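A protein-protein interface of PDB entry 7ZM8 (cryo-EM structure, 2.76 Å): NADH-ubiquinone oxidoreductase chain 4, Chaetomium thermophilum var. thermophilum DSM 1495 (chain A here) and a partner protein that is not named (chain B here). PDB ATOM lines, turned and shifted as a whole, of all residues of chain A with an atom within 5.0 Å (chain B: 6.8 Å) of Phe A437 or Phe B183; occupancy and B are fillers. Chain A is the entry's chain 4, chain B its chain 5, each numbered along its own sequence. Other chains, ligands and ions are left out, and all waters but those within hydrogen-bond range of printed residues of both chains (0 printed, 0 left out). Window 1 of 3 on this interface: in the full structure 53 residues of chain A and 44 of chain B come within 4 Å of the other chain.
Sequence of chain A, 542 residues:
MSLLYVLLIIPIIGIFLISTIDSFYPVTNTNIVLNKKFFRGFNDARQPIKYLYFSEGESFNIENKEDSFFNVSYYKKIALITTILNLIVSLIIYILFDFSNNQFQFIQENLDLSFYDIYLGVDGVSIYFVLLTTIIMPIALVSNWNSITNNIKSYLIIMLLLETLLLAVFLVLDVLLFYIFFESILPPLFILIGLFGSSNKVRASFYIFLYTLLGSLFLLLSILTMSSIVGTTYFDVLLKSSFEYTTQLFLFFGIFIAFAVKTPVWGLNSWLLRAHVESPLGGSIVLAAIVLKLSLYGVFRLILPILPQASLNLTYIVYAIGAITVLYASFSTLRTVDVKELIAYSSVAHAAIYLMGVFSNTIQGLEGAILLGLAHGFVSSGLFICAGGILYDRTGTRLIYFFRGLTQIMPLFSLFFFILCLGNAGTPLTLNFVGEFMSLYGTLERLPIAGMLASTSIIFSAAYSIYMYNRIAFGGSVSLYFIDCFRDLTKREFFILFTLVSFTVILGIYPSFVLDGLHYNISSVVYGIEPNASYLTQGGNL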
ATOM      1  N   PHE A 433      38.158  12.076 -19.140  1.00  0.00           N
ATOM      2  CA  PHE A 433      36.875  12.771 -18.868  1.00  0.00           C
ATOM      3  C   PHE A 433      36.047  12.001 -17.836  1.00  0.00           C
ATOM      4  O   PHE A 433      35.527  12.642 -16.917  1.00  0.00           O
ATOM      5  CB  PHE A 433      36.090  13.021 -20.156  1.00  0.00           C
ATOM      6  CG  PHE A 433      34.677  13.493 -19.925  1.00  0.00           C
ATOM      7  CD1 PHE A 433      34.428  14.778 -19.468  1.00  0.00           C
ATOM      8  CD2 PHE A 433      33.599  12.650 -20.141  1.00  0.00           C
ATOM      9  CE1 PHE A 433      33.131  15.207 -19.236  1.00  0.00           C
ATOM     10  CE2 PHE A 433      32.304  13.082 -19.911  1.00  0.00           C
ATOM     11  CZ  PHE A 433      32.073  14.359 -19.460  1.00  0.00           C
ATOM     12  N   VAL A 434      35.959  10.675 -17.967  1.00  0.00           N
ATOM     13  CA  VAL A 434      35.091   9.872 -17.056  1.00  0.00           C
ATOM     14  C   VAL A 434      35.606   9.999 -15.623  1.00  0.00           C
ATOM     15  O   VAL A 434      34.784  10.236 -14.725  1.00  0.00           O
ATOM     16  CB  VAL A 434      35.044   8.398 -17.500  1.00  0.00           C
ATOM     17  CG1 VAL A 434      34.036   7.595 -16.694  1.00  0.00           C
ATOM     18  CG2 VAL A 434      34.764   8.272 -18.988  1.00  0.00           C
ATOM     19  N   GLY A 435      36.924   9.886 -15.432  1.00  0.00           N
ATOM     20  CA  GLY A 435      37.505   9.944 -14.082  1.00  0.00           C
ATOM     21  C   GLY A 435      37.293  11.294 -13.449  1.00  0.00           C
ATOM     22  O   GLY A 435      36.906  11.334 -12.286  1.00  0.00           O
ATOM     23  N   GLU A 436      37.507  12.361 -14.210  1.00  0.00           N
ATOM     24  CA  GLU A 436      37.347  13.742 -13.694  1.00  0.00           C
ATOM     25  C   GLU A 436      35.886  13.969 -13.320  1.00  0.00           C
ATOM     26  O   GLU A 436      35.654  14.506 -12.243  1.00  0.00           O
ATOM     27  CB  GLU A 436      37.803  14.730 -14.764  1.00  0.00           C
ATOM     28  CG  GLU A 436      37.777  16.181 -14.325  1.00  0.00           C
ATOM     29  CD  GLU A 436      39.130  16.730 -13.915  1.00  0.00           C
ATOM     30  OE1 GLU A 436      40.083  15.937 -13.826  1.00  0.00           O
ATOM     31  OE2 GLU A 436      39.229  17.950 -13.699  1.00  0.00           O
ATOM     32  N   PHE A 437      34.945  13.536 -14.157  1.00  0.00           N
ATOM     33  CA  PHE A 437      33.509  13.795 -13.908  1.00  0.00           C
ATOM     34  C   PHE A 437      33.069  13.113 -12.616  1.00  0.00           C
ATOM     35  O   PHE A 437      32.410  13.758 -11.796  1.00  0.00           O
ATOM     36  CB  PHE A 437      32.702  13.227 -15.076  1.00  0.00           C
ATOM     37  CG  PHE A 437      31.283  13.724 -15.177  1.00  0.00           C
ATOM     38  CD1 PHE A 437      31.006  14.970 -15.715  1.00  0.00           C
ATOM     39  CD2 PHE A 437      30.225  12.945 -14.740  1.00  0.00           C
ATOM     40  CE1 PHE A 437      29.702  15.431 -15.804  1.00  0.00           C
ATOM     41  CE2 PHE A 437      28.923  13.407 -14.829  1.00  0.00           C
ATOM     42  CZ  PHE A 437      28.663  14.648 -15.361  1.00  0.00           C
ATOM     43  N   MET A 438      33.425  11.841 -12.451  1.00  0.00           N
ATOM     44  CA  MET A 438      33.057  11.075 -11.235  1.00  0.00           C
ATOM     45  C   MET A 438      33.840  11.582 -10.022  1.00  0.00           C
ATOM     46  O   MET A 438      33.247  11.671  -8.943  1.00  0.00           O
ATOM     47  CB  MET A 438      33.282   9.582 -11.470  1.00  0.00           C
ATOM     48  CG  MET A 438      32.322   8.977 -12.473  1.00  0.00           C
ATOM     49  SD  MET A 438      32.781   7.289 -12.944  1.00  0.00           S
ATOM     50  CE  MET A 438      32.442   6.406 -11.423  1.00  0.00           C
ATOM     51  N   SER A 439      35.120  11.903 -10.202  1.00  0.00           N
ATOM     52  CA  SER A 439      35.935  12.472  -9.097  1.00  0.00           C
ATOM     53  C   SER A 439      35.346  13.817  -8.686  1.00  0.00           C
ATOM     54  O   SER A 439      35.312  14.092  -7.486  1.00  0.00           O
ATOM     55  CB  SER A 439      37.376  12.631  -9.476  1.00  0.00           C
ATOM     56  OG  SER A 439      38.062  11.396  -9.432  1.00  0.00           O
ATOM     57  N   LEU A 440      34.862  14.596  -9.648  1.00  0.00           N
ATOM     58  CA  LEU A 440      34.377  15.963  -9.347  1.00  0.00           C
ATOM     59  C   LEU A 440      32.983  15.881  -8.742  1.00  0.00           C
ATOM     60  O   LEU A 440      32.645  16.761  -7.936  1.00  0.00           O
ATOM     61  CB  LEU A 440      34.402  16.836 -10.604  1.00  0.00           C
ATOM     62  CG  LEU A 440      35.757  17.443 -10.956  1.00  0.00           C
ATOM     63  CD1 LEU A 440      35.626  18.406 -12.122  1.00  0.00           C
ATOM     64  CD2 LEU A 440      36.361  18.143  -9.751  1.00  0.00           C
ATOM     65  N   TYR A 441      32.216  14.857  -9.112  1.00  0.00           N
ATOM     66  CA  TYR A 441      30.827  14.778  -8.609  1.00  0.00           C
ATOM     67  C   TYR A 441      30.862  14.361  -7.146  1.00  0.00           C
ATOM     68  O   TYR A 441      30.142  14.975  -6.355  1.00  0.00           O
ATOM     69  CB  TYR A 441      30.016  13.725  -9.364  1.00  0.00           C
ATOM     70  CG  TYR A 441      28.748  13.305  -8.661  1.00  0.00           C
ATOM     71  CD1 TYR A 441      27.601  14.077  -8.738  1.00  0.00           C
ATOM     72  CD2 TYR A 441      28.697  12.153  -7.895  1.00  0.00           C
ATOM     73  CE1 TYR A 441      26.442  13.713  -8.076  1.00  0.00           C
ATOM     74  CE2 TYR A 441      27.551  11.783  -7.215  1.00  0.00           C
ATOM     75  CZ  TYR A 441      26.416  12.565  -7.310  1.00  0.00           C
ATOM     76  OH  TYR A 441      25.273  12.198  -6.663  1.00  0.00           O
ATOM     77  N   LEU A 444      31.769  17.327  -5.060  1.00  0.00           N
ATOM     78  CA  LEU A 444      30.606  18.240  -4.877  1.00  0.00           C
ATOM     79  C   LEU A 444      29.580  17.657  -3.898  1.00  0.00           C
ATOM     80  O   LEU A 444      28.988  18.420  -3.148  1.00  0.00           O
ATOM     81  CB  LEU A 444      29.979  18.522  -6.248  1.00  0.00           C
ATOM     82  CG  LEU A 444      29.031  19.718  -6.296  1.00  0.00           C
ATOM     83  CD1 LEU A 444      29.705  20.906  -6.960  1.00  0.00           C
ATOM     84  CD2 LEU A 444      27.744  19.359  -7.021  1.00  0.00           C
ATOM     85  N   ILE B  65      28.633   4.769 -18.986  1.00  0.00           N
ATOM     86  CA  ILE B  65      29.092   4.886 -17.607  1.00  0.00           C
ATOM     87  C   ILE B  65      28.125   4.128 -16.710  1.00  0.00           C
ATOM     88  O   ILE B  65      26.918   4.379 -16.741  1.00  0.00           O
ATOM     89  CB  ILE B  65      29.215   6.357 -17.173  1.00  0.00           C
ATOM     90  CG1 ILE B  65      30.160   7.103 -18.109  1.00  0.00           C
ATOM     91  CG2 ILE B  65      29.719   6.454 -15.746  1.00  0.00           C
ATOM     92  CD1 ILE B  65      29.742   8.510 -18.395  1.00  0.00           C
ATOM     93  N   PHE B  70      23.988   5.568 -11.404  1.00  0.00           N
ATOM     94  CA  PHE B  70      24.444   6.192 -12.639  1.00  0.00           C
ATOM     95  C   PHE B  70      24.492   5.123 -13.719  1.00  0.00           C
ATOM     96  O   PHE B  70      25.325   4.215 -13.661  1.00  0.00           O
ATOM     97  CB  PHE B  70      25.822   6.843 -12.488  1.00  0.00           C
ATOM     98  CG  PHE B  70      25.868   8.020 -11.547  1.00  0.00           C
ATOM     99  CD1 PHE B  70      24.791   8.348 -10.739  1.00  0.00           C
ATOM    100  CD2 PHE B  70      27.003   8.809 -11.483  1.00  0.00           C
ATOM    101  CE1 PHE B  70      24.848   9.423  -9.878  1.00  0.00           C
ATOM    102  CE2 PHE B  70      27.061   9.892 -10.624  1.00  0.00           C
ATOM    103  CZ  PHE B  70      25.979  10.196  -9.823  1.00  0.00           C
ATOM    104  N   LEU B 134      24.581  13.753 -20.538  1.00  0.00           N
ATOM    105  CA  LEU B 134      26.012  13.488 -20.598  1.00  0.00           C
ATOM    106  C   LEU B 134      26.468  13.095 -21.996  1.00  0.00           C
ATOM    107  O   LEU B 134      27.581  13.446 -22.396  1.00  0.00           O
ATOM    108  CB  LEU B 134      26.393  12.409 -19.584  1.00  0.00           C
ATOM    109  CG  LEU B 134      27.833  12.406 -19.062  1.00  0.00           C
ATOM    110  CD1 LEU B 134      28.322  13.807 -18.748  1.00  0.00           C
ATOM    111  CD2 LEU B 134      27.910  11.547 -17.834  1.00  0.00           C
ATOM    112  N   PHE B 137      26.527  16.294 -23.913  1.00  0.00           N
ATOM    113  CA  PHE B 137      27.794  17.003 -23.616  1.00  0.00           C
ATOM    114  C   PHE B 137      28.927  16.517 -24.536  1.00  0.00           C
ATOM    115  O   PHE B 137      29.810  17.312 -24.830  1.00  0.00           O
ATOM    116  CB  PHE B 137      28.096  16.910 -22.121  1.00  0.00           C
ATOM    117  CG  PHE B 137      29.208  17.799 -21.633  1.00  0.00           C
ATOM    118  CD1 PHE B 137      29.030  19.169 -21.549  1.00  0.00           C
ATOM    119  CD2 PHE B 137      30.421  17.264 -21.236  1.00  0.00           C
ATOM    120  CE1 PHE B 137      30.043  19.988 -21.083  1.00  0.00           C
ATOM    121  CE2 PHE B 137      31.436  18.086 -20.775  1.00  0.00           C
ATOM    122  CZ  PHE B 137      31.242  19.444 -20.696  1.00  0.00           C
ATOM    123  N   CYS B 176      32.165  24.364 -17.813  1.00  0.00           N
ATOM    124  CA  CYS B 176      32.314  24.235 -16.346  1.00  0.00           C
ATOM    125  C   CYS B 176      30.939  24.352 -15.691  1.00  0.00           C
ATOM    126  O   CYS B 176      30.669  23.577 -14.765  1.00  0.00           O
ATOM    127  CB  CYS B 176      33.226  25.323 -15.793  1.00  0.00           C
ATOM    128  SG  CYS B 176      33.621  25.138 -14.037  1.00  0.00           S
ATOM    129  N   PHE B 177      30.108  25.276 -16.170  1.00  0.00           N
ATOM    130  CA  PHE B 177      28.813  25.477 -15.539  1.00  0.00           C
ATOM    131  C   PHE B 177      27.814  24.382 -15.900  1.00  0.00           C
ATOM    132  O   PHE B 177      27.007  23.993 -15.050  1.00  0.00           O
ATOM    133  CB  PHE B 177      28.281  26.857 -15.909  1.00  0.00           C
ATOM    134  CG  PHE B 177      28.806  27.943 -15.027  1.00  0.00           C
ATOM    135  CD1 PHE B 177      28.258  28.161 -13.777  1.00  0.00           C
ATOM    136  CD2 PHE B 177      29.885  28.710 -15.422  1.00  0.00           C
ATOM    137  CE1 PHE B 177      28.755  29.151 -12.954  1.00  0.00           C
ATOM    138  CE2 PHE B 177      30.384  29.700 -14.604  1.00  0.00           C
ATOM    139  CZ  PHE B 177      29.819  29.921 -13.369  1.00  0.00           C
ATOM    140  N   LEU B 178      27.852  23.863 -17.130  1.00  0.00           N
ATOM    141  CA  LEU B 178      27.047  22.688 -17.440  1.00  0.00           C
ATOM    142  C   LEU B 178      27.474  21.484 -16.618  1.00  0.00           C
ATOM    143  O   LEU B 178      26.633  20.676 -16.207  1.00  0.00           O
ATOM    144  CB  LEU B 178      27.119  22.333 -18.919  1.00  0.00           C
ATOM    145  CG  LEU B 178      26.437  23.221 -19.937  1.00  0.00           C
ATOM    146  CD1 LEU B 178      26.692  22.614 -21.275  1.00  0.00           C
ATOM    147  CD2 LEU B 178      24.961  23.291 -19.648  1.00  0.00           C
ATOM    148  N   THR B 179      28.777  21.321 -16.403  1.00  0.00           N
ATOM    149  CA  THR B 179      29.242  20.198 -15.601  1.00  0.00           C
ATOM    150  C   THR B 179      28.734  20.314 -14.169  1.00  0.00           C
ATOM    151  O   THR B 179      28.339  19.315 -13.559  1.00  0.00           O
ATOM    152  CB  THR B 179      30.768  20.123 -15.652  1.00  0.00           C
ATOM    153  OG1 THR B 179      31.186  19.938 -17.007  1.00  0.00           O
ATOM    154  CG2 THR B 179      31.279  18.958 -14.841  1.00  0.00           C
ATOM    155  N   VAL B 180      28.721  21.530 -13.625  1.00  0.00           N
ATOM    156  CA  VAL B 180      28.109  21.766 -12.322  1.00  0.00           C
ATOM    157  C   VAL B 180      26.608  21.525 -12.386  1.00  0.00           C
ATOM    158  O   VAL B 180      26.017  20.961 -11.460  1.00  0.00           O
ATOM    159  CB  VAL B 180      28.433  23.190 -11.835  1.00  0.00           C
ATOM    160  CG1 VAL B 180      27.584  23.551 -10.637  1.00  0.00           C
ATOM    161  CG2 VAL B 180      29.901  23.309 -11.502  1.00  0.00           C
ATOM    162  N   GLY B 181      25.964  21.962 -13.468  1.00  0.00           N
ATOM    163  CA  GLY B 181      24.536  21.748 -13.607  1.00  0.00           C
ATOM    164  C   GLY B 181      24.151  20.291 -13.755  1.00  0.00           C
ATOM    165  O   GLY B 181      23.108  19.873 -13.248  1.00  0.00           O
ATOM    166  N   MET B 182      24.969  19.505 -14.459  1.00  0.00           N
ATOM    167  CA  MET B 182      24.710  18.070 -14.552  1.00  0.00           C
ATOM    168  C   MET B 182      25.022  17.354 -13.248  1.00  0.00           C
ATOM    169  O   MET B 182      24.396  16.334 -12.948  1.00  0.00           O
ATOM    170  CB  MET B 182      25.496  17.439 -15.702  1.00  0.00           C
ATOM    171  CG  MET B 182      25.063  17.893 -17.086  1.00  0.00           C
ATOM    172  SD  MET B 182      25.951  17.080 -18.433  1.00  0.00           S
ATOM    173  CE  MET B 182      27.556  17.869 -18.369  1.00  0.00           C
ATOM    174  N   PHE B 183      25.985  17.855 -12.472  1.00  0.00           N
ATOM    175  CA  PHE B 183      26.215  17.301 -11.142  1.00  0.00           C
ATOM    176  C   PHE B 183      24.994  17.488 -10.261  1.00  0.00           C
ATOM    177  O   PHE B 183      24.630  16.592  -9.493  1.00  0.00           O
ATOM    178  CB  PHE B 183      27.435  17.948 -10.485  1.00  0.00           C
ATOM    179  CG  PHE B 183      28.739  17.540 -11.086  1.00  0.00           C
ATOM    180  CD1 PHE B 183      28.839  16.401 -11.860  1.00  0.00           C
ATOM    181  CD2 PHE B 183      29.873  18.296 -10.872  1.00  0.00           C
ATOM    182  CE1 PHE B 183      30.038  16.033 -12.415  1.00  0.00           C
ATOM    183  CE2 PHE B 183      31.074  17.931 -11.430  1.00  0.00           C
ATOM    184  CZ  PHE B 183      31.155  16.792 -12.200  1.00  0.00           C
ATOM    185  N   ALA B 184      24.367  18.664 -10.384  1.00  0.00           N
ATOM    186  CA  ALA B 184      23.156  18.972  -9.596  1.00  0.00           C
ATOM    187  C   ALA B 184      22.030  18.005  -9.953  1.00  0.00           C
ATOM    188  O   ALA B 184      21.293  17.625  -9.052  1.00  0.00           O
ATOM    189  CB  ALA B 184      22.752  20.403  -9.808  1.00  0.00           C
ATOM    190  N   ILE B 185      21.889  17.681 -11.243  1.00  0.00           N
ATOM    191  CA  ILE B 185      20.842  16.768 -11.694  1.00  0.00           C
ATOM    192  C   ILE B 185      21.090  15.365 -11.156  1.00  0.00           C
ATOM    193  O   ILE B 185      20.179  14.719 -10.627  1.00  0.00           O
ATOM    194  CB  ILE B 185      20.751  16.776 -13.232  1.00  0.00           C
ATOM    195  CG1 ILE B 185      20.317  18.146 -13.744  1.00  0.00           C
ATOM    196  CG2 ILE B 185      19.792  15.717 -13.724  1.00  0.00           C
ATOM    197  CD1 ILE B 185      20.352  18.262 -15.251  1.00  0.00           C
ATOM    198  N   LEU B 186      22.327  14.874 -11.277  1.00  0.00           N
ATOM    199  CA  LEU B 186      22.667  13.568 -10.717  1.00  0.00           C
ATOM    200  C   LEU B 186      22.491  13.556  -9.207  1.00  0.00           C
ATOM    201  O   LEU B 186      21.982  12.583  -8.641  1.00  0.00           O
ATOM    202  CB  LEU B 186      24.107  13.194 -11.066  1.00  0.00           C
ATOM    203  CG  LEU B 186      24.483  12.827 -12.498  1.00  0.00           C
ATOM    204  CD1 LEU B 186      25.982  12.941 -12.671  1.00  0.00           C
ATOM    205  CD2 LEU B 186      24.005  11.432 -12.869  1.00  0.00           C
ATOM    206  N   TRP B 187      22.862  14.639  -8.523  1.00  0.00           N
ATOM    207  CA  TRP B 187      22.757  14.726  -7.045  1.00  0.00           C
ATOM    208  C   TRP B 187      21.291  14.711  -6.617  1.00  0.00           C
ATOM    209  O   TRP B 187      20.996  14.022  -5.666  1.00  0.00           O
ATOM    210  CB  TRP B 187      23.523  15.937  -6.516  1.00  0.00           C
ATOM    211  CG  TRP B 187      23.736  15.959  -5.036  1.00  0.00           C
ATOM    212  CD1 TRP B 187      23.483  14.958  -4.144  1.00  0.00           C
ATOM    213  CD2 TRP B 187      24.258  17.054  -4.267  1.00  0.00           C
ATOM    214  NE1 TRP B 187      23.802  15.359  -2.877  1.00  0.00           N
ATOM    215  CE2 TRP B 187      24.282  16.640  -2.921  1.00  0.00           C
ATOM    216  CE3 TRP B 187      24.707  18.339  -4.587  1.00  0.00           C
ATOM    217  CZ2 TRP B 187      24.740  17.464  -1.897  1.00  0.00           C
ATOM    218  CZ3 TRP B 187      25.155  19.153  -3.574  1.00  0.00           C
ATOM    219  CH2 TRP B 187      25.165  18.720  -2.250  1.00  0.00           C
ATOM    220  N   SER B 188      20.426  15.455  -7.289  1.00  0.00           N
ATOM    221  CA  SER B 188      18.974  15.467  -6.985  1.00  0.00           C
ATOM    222  C   SER B 188      18.200  14.229  -7.433  1.00  0.00           C
ATOM    223  O   SER B 188      17.468  13.675  -6.599  1.00  0.00           O
ATOM    224  CB  SER B 188      18.321  16.680  -7.558  1.00  0.00           C
ATOM    225  OG  SER B 188      18.172  16.572  -8.959  1.00  0.00           O
ATOM    226  N   LEU B 192      20.913  11.383 -15.074  1.00  0.00           N
ATOM    227  CA  LEU B 192      20.578  12.460 -16.001  1.00  0.00           C
ATOM    228  C   LEU B 192      20.087  11.976 -17.366  1.00  0.00           C
ATOM    229  O   LEU B 192      20.542  12.438 -18.399  1.00  0.00           O
ATOM    230  CB  LEU B 192      21.783  13.392 -16.107  1.00  0.00           C
ATOM    231  CG  LEU B 192      23.168  12.838 -16.466  1.00  0.00           C
ATOM    232  CD1 LEU B 192      23.393  12.619 -17.917  1.00  0.00           C
ATOM    233  CD2 LEU B 192      24.214  13.784 -15.941  1.00  0.00           C
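Among the printed residues, pairs that only touch across the chains: Phe A433 with Leu B134, Phe A433 with Phe B137, Phe A437 with Leu B134, Phe A437 with Thr B179, Phe A437 with Phe B183, Phe A437 with Leu B186, Leu A440 with Phe B183, Tyr A441 with Phe B70, Tyr A441 with Phe B183, Tyr A441 with Leu B186, Tyr A441 with Trp B187, Leu A444 with Phe B183 and Leu A444 with Trp B187.
Printed residues of chain B within 4 Å of Phe A437: Leu B134, Thr B179, Phe B183 and Leu B186. Of the printed residues of chain B, Tyr A441 touches Phe B70 (3.4 Å), Phe B183 (3.7 Å), Leu B186 (3.8 Å) and Trp B187 (3.6 Å). Leu B178 touches none of the printed residues of chain A. Gly B181 touches none of the printed residues of chain A. Phe B183 touches four residues of chain A. Of the printed residues of chain A, Trp B187 touches Tyr A441 and Leu A444. The nearest printed residue of chain B that does not touch Phe A437 is Met B182 (4.1 Å).
Hydrophobic or aromatic side chains of chain B within 4 Å of the printed part of chain A: Phe B70, Leu B134, Phe B137, Phe B183, Leu B186 and Trp B187. Of the 10 printed residues of chain A, 5 touch a printed residue of chain B.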
